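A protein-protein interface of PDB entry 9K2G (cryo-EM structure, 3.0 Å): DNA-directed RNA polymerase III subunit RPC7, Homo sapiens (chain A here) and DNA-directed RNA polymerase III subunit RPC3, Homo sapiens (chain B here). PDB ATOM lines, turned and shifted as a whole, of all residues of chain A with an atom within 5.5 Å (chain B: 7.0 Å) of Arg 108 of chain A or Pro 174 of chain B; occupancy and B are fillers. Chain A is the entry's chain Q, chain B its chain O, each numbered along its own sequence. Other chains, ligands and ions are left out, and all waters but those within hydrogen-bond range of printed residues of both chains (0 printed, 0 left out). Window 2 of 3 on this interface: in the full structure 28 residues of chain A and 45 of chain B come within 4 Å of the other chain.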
ATOM      1  N   LEU A 106      25.454  31.123   3.454  1.00  0.00           N
ATOM      2  CA  LEU A 106      24.694  31.454   2.256  1.00  0.00           C
ATOM      3  C   LEU A 106      25.333  30.807   1.032  1.00  0.00           C
ATOM      4  O   LEU A 106      26.563  30.738   0.937  1.00  0.00           O
ATOM      5  CB  LEU A 106      24.628  32.975   2.085  1.00  0.00           C
ATOM      6  CG  LEU A 106      23.665  33.554   1.054  1.00  0.00           C
ATOM      7  CD1 LEU A 106      22.222  33.249   1.422  1.00  0.00           C
ATOM      8  CD2 LEU A 106      23.875  35.046   0.932  1.00  0.00           C
ATOM      9  N   PRO A 107      24.532  30.309   0.089  1.00  0.00           N
ATOM     10  CA  PRO A 107      25.103  29.759  -1.141  1.00  0.00           C
ATOM     11  C   PRO A 107      25.881  30.810  -1.920  1.00  0.00           C
ATOM     12  O   PRO A 107      25.686  32.020  -1.761  1.00  0.00           O
ATOM     13  CB  PRO A 107      23.874  29.280  -1.923  1.00  0.00           C
ATOM     14  CG  PRO A 107      22.867  28.977  -0.869  1.00  0.00           C
ATOM     15  CD  PRO A 107      23.102  29.985   0.230  1.00  0.00           C
ATOM     16  N   ARG A 108      26.781  30.327  -2.776  1.00  0.00           N
ATOM     17  CA  ARG A 108      27.738  31.188  -3.460  1.00  0.00           C
ATOM     18  C   ARG A 108      27.084  32.189  -4.406  1.00  0.00           C
ATOM     19  O   ARG A 108      27.709  33.192  -4.759  1.00  0.00           O
ATOM     20  CB  ARG A 108      28.738  30.338  -4.250  1.00  0.00           C
ATOM     21  CG  ARG A 108      28.085  29.551  -5.378  1.00  0.00           C
ATOM     22  CD  ARG A 108      28.999  29.435  -6.587  1.00  0.00           C
ATOM     23  NE  ARG A 108      30.153  28.587  -6.323  1.00  0.00           N
ATOM     24  CZ  ARG A 108      30.167  27.272  -6.485  1.00  0.00           C
ATOM     25  NH1 ARG A 108      29.097  26.617  -6.904  1.00  0.00           N
ATOM     26  NH2 ARG A 108      31.282  26.595  -6.224  1.00  0.00           N
ATOM     27  N   GLU A 109      25.852  31.929  -4.843  1.00  0.00           N
ATOM     28  CA  GLU A 109      25.257  32.718  -5.919  1.00  0.00           C
ATOM     29  C   GLU A 109      24.875  34.134  -5.512  1.00  0.00           C
ATOM     30  O   GLU A 109      24.569  34.945  -6.391  1.00  0.00           O
ATOM     31  CB  GLU A 109      24.030  31.991  -6.469  1.00  0.00           C
ATOM     32  CG  GLU A 109      24.306  30.586  -6.982  1.00  0.00           C
ATOM     33  CD  GLU A 109      23.040  29.853  -7.369  1.00  0.00           C
ATOM     34  OE1 GLU A 109      21.945  30.338  -7.018  1.00  0.00           O
ATOM     35  OE2 GLU A 109      23.136  28.792  -8.025  1.00  0.00           O
ATOM     36  N   MET A 110      24.881  34.462  -4.221  1.00  0.00           N
ATOM     37  CA  MET A 110      24.318  35.719  -3.750  1.00  0.00           C
ATOM     38  C   MET A 110      25.370  36.738  -3.318  1.00  0.00           C
ATOM     39  O   MET A 110      25.010  37.772  -2.740  1.00  0.00           O
ATOM     40  CB  MET A 110      23.335  35.469  -2.608  1.00  0.00           C
ATOM     41  CG  MET A 110      21.966  35.007  -3.077  1.00  0.00           C
ATOM     42  SD  MET A 110      21.984  33.328  -3.725  1.00  0.00           S
ATOM     43  CE  MET A 110      22.111  32.398  -2.206  1.00  0.00           C
ATOM     44  N   MET A 111      26.649  36.487  -3.572  1.00  0.00           N
ATOM     45  CA  MET A 111      27.638  37.536  -3.375  1.00  0.00           C
ATOM     46  C   MET A 111      27.455  38.619  -4.441  1.00  0.00           C
ATOM     47  O   MET A 111      27.169  38.303  -5.599  1.00  0.00           O
ATOM     48  CB  MET A 111      29.060  36.979  -3.421  1.00  0.00           C
ATOM     49  CG  MET A 111      29.560  36.452  -2.084  1.00  0.00           C
ATOM     50  SD  MET A 111      29.075  34.743  -1.780  1.00  0.00           S
ATOM     51  CE  MET A 111      30.208  33.861  -2.853  1.00  0.00           C
ATOM     52  N   ARG A 113      29.587  40.511  -5.981  1.00  0.00           N
ATOM     53  CA  ARG A 113      30.671  40.592  -6.967  1.00  0.00           C
ATOM     54  C   ARG A 113      30.807  42.012  -7.515  1.00  0.00           C
ATOM     55  O   ARG A 113      31.912  42.471  -7.810  1.00  0.00           O
ATOM     56  CB  ARG A 113      30.459  39.605  -8.118  1.00  0.00           C
ATOM     57  CG  ARG A 113      30.892  38.181  -7.816  1.00  0.00           C
ATOM     58  CD  ARG A 113      29.760  37.367  -7.224  1.00  0.00           C
ATOM     59  NE  ARG A 113      28.703  37.129  -8.202  1.00  0.00           N
ATOM     60  CZ  ARG A 113      27.552  36.530  -7.929  1.00  0.00           C
ATOM     61  NH1 ARG A 113      27.268  36.100  -6.708  1.00  0.00           N
ATOM     62  NH2 ARG A 113      26.662  36.362  -8.902  1.00  0.00           N
ATOM     63  N   GLY B  71      22.807  19.752  -9.202  1.00  0.00           N
ATOM     64  CA  GLY B  71      23.340  20.746  -8.285  1.00  0.00           C
ATOM     65  C   GLY B  71      22.615  22.074  -8.271  1.00  0.00           C
ATOM     66  O   GLY B  71      23.174  23.065  -7.803  1.00  0.00           O
ATOM     67  N   TYR B  75      14.731  27.468  -3.651  1.00  0.00           N
ATOM     68  CA  TYR B  75      14.340  28.182  -2.445  1.00  0.00           C
ATOM     69  C   TYR B  75      12.854  27.982  -2.192  1.00  0.00           C
ATOM     70  O   TYR B  75      12.028  28.224  -3.077  1.00  0.00           O
ATOM     71  CB  TYR B  75      14.667  29.675  -2.567  1.00  0.00           C
ATOM     72  CG  TYR B  75      16.091  29.955  -2.981  1.00  0.00           C
ATOM     73  CD1 TYR B  75      17.100  30.065  -2.030  1.00  0.00           C
ATOM     74  CD2 TYR B  75      16.432  30.107  -4.317  1.00  0.00           C
ATOM     75  CE1 TYR B  75      18.406  30.319  -2.403  1.00  0.00           C
ATOM     76  CE2 TYR B  75      17.733  30.360  -4.700  1.00  0.00           C
ATOM     77  CZ  TYR B  75      18.716  30.465  -3.739  1.00  0.00           C
ATOM     78  OH  TYR B  75      20.013  30.719  -4.117  1.00  0.00           O
ATOM     79  N   ASP B 170      34.120  15.824   2.177  1.00  0.00           N
ATOM     80  CA  ASP B 170      34.324  15.967   0.739  1.00  0.00           C
ATOM     81  C   ASP B 170      35.261  17.126   0.416  1.00  0.00           C
ATOM     82  O   ASP B 170      34.815  18.152  -0.110  1.00  0.00           O
ATOM     83  CB  ASP B 170      32.981  16.158   0.031  1.00  0.00           C
ATOM     84  CG  ASP B 170      33.080  15.974  -1.470  1.00  0.00           C
ATOM     85  OD1 ASP B 170      34.163  15.585  -1.956  1.00  0.00           O
ATOM     86  OD2 ASP B 170      32.075  16.220  -2.168  1.00  0.00           O
ATOM     87  N   GLY B 172      37.506  19.281  -1.760  1.00  0.00           N
ATOM     88  CA  GLY B 172      37.656  19.440  -3.190  1.00  0.00           C
ATOM     89  C   GLY B 172      36.777  20.543  -3.741  1.00  0.00           C
ATOM     90  O   GLY B 172      36.769  21.674  -3.240  1.00  0.00           O
ATOM     91  N   PRO B 173      36.031  20.242  -4.802  1.00  0.00           N
ATOM     92  CA  PRO B 173      35.148  21.246  -5.408  1.00  0.00           C
ATOM     93  C   PRO B 173      34.104  21.727  -4.416  1.00  0.00           C
ATOM     94  O   PRO B 173      33.545  20.927  -3.649  1.00  0.00           O
ATOM     95  CB  PRO B 173      34.499  20.486  -6.573  1.00  0.00           C
ATOM     96  CG  PRO B 173      35.428  19.353  -6.860  1.00  0.00           C
ATOM     97  CD  PRO B 173      36.003  18.963  -5.533  1.00  0.00           C
ATOM     98  N   PRO B 174      33.817  23.027  -4.394  1.00  0.00           N
ATOM     99  CA  PRO B 174      32.814  23.550  -3.470  1.00  0.00           C
ATOM    100  C   PRO B 174      31.409  23.366  -4.023  1.00  0.00           C
ATOM    101  O   PRO B 174      31.145  23.681  -5.193  1.00  0.00           O
ATOM    102  CB  PRO B 174      33.179  25.036  -3.356  1.00  0.00           C
ATOM    103  CG  PRO B 174      33.832  25.352  -4.659  1.00  0.00           C
ATOM    104  CD  PRO B 174      34.532  24.096  -5.113  1.00  0.00           C
ATOM    105  N   PRO B 175      30.483  22.848  -3.213  1.00  0.00           N
ATOM    106  CA  PRO B 175      29.112  22.685  -3.688  1.00  0.00           C
ATOM    107  C   PRO B 175      28.437  24.031  -3.856  1.00  0.00           C
ATOM    108  O   PRO B 175      28.833  25.023  -3.224  1.00  0.00           O
ATOM    109  CB  PRO B 175      28.448  21.857  -2.571  1.00  0.00           C
ATOM    110  CG  PRO B 175      29.240  22.183  -1.352  1.00  0.00           C
ATOM    111  CD  PRO B 175      30.655  22.375  -1.828  1.00  0.00           C
ATOM    112  N   PRO B 176      27.415  24.123  -4.715  1.00  0.00           N
ATOM    113  CA  PRO B 176      26.685  25.394  -4.847  1.00  0.00           C
ATOM    114  C   PRO B 176      26.067  25.856  -3.541  1.00  0.00           C
ATOM    115  O   PRO B 176      26.013  27.065  -3.276  1.00  0.00           O
ATOM    116  CB  PRO B 176      25.619  25.081  -5.908  1.00  0.00           C
ATOM    117  CG  PRO B 176      26.157  23.896  -6.651  1.00  0.00           C
ATOM    118  CD  PRO B 176      26.912  23.094  -5.642  1.00  0.00           C
ATOM    119  N   ALA B 177      25.595  24.924  -2.717  1.00  0.00           N
ATOM    120  CA  ALA B 177      25.085  25.223  -1.394  1.00  0.00           C
ATOM    121  C   ALA B 177      25.804  24.346  -0.376  1.00  0.00           C
ATOM    122  O   ALA B 177      26.031  23.162  -0.630  1.00  0.00           O
ATOM    123  CB  ALA B 177      23.572  24.986  -1.312  1.00  0.00           C
ATOM    124  N   PRO B 178      26.175  24.905   0.781  1.00  0.00           N
ATOM    125  CA  PRO B 178      26.929  24.123   1.772  1.00  0.00           C
ATOM    126  C   PRO B 178      26.123  23.036   2.459  1.00  0.00           C
ATOM    127  O   PRO B 178      26.704  22.269   3.239  1.00  0.00           O
ATOM    128  CB  PRO B 178      27.393  25.188   2.778  1.00  0.00           C
ATOM    129  CG  PRO B 178      26.408  26.288   2.638  1.00  0.00           C
ATOM    130  CD  PRO B 178      25.982  26.303   1.202  1.00  0.00           C
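Printed residues of chain B within 4 Å of Arg 108 of chain A: Pro 174 and Pro 176. Printed residues of chain B within 4 Å of Glu 109 of chain A: Tyr 75 (3.5 Å). Of the printed residues of chain A, Tyr 75 of chain B touches Glu 109 (3.5 Å) and Met 110 (3.3 Å). Asp 170 of chain B touches none of the printed residues of chain A. Gly 172 of chain B touches none of the printed residues of chain A. Of chain A, only Arg 108 comes within 4 Å of Pro 174 of chain B. The nearest printed residue of chain A that does not touch Pro 174 of chain B is Met 111 of chain A (9.3 Å). The nearest printed residue of chain B that does not touch Pro 107 of chain A is Ala 177 of chain B (4.1 Å).
Pro 107 of chain A touches Pro 176 of chain B (CB to O, 3.4 Å). Tyr 75 of chain B touches Glu 109 of chain A (OH to OE1, 3.5 Å).
SD of Met 110 of chain A sits at hydrogen-bond distance from OH of Tyr 75 of chain B (3.3 Å). The backbone carbonyl oxygen (O) of Pro 174 of chain B is in hydrogen-bond range of the guanidinium group (NH2) of Arg 108 of chain A (3.1 Å). N of Arg 108 of chain A lies within hydrogen-bond range of O of Pro 176 of chain B (3.4 Å).
Hydrophobic or aromatic side chains of chain B within 4 Å of the printed part of chain A: Tyr 75, Pro 174 and Pro 176. Of the 7 printed residues of chain A, 4 touch a printed residue of chain B. Hydrophobic or aromatic side chains of chain A that line the printed part of chain B: Pro 107 and Met 110. Among the printed residues, 5 pairs touch across the chains. Among the printed residues, no Asp or Glu carboxylate lies within 4 Å of a Lys or Arg side-chain nitrogen of the other chain.
The backbone carbonyl oxygen of Glu 109 of chain A sits at hydrogen-bond distance from the guanidinium group of Arg 113 of chain A (3.0 Å).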
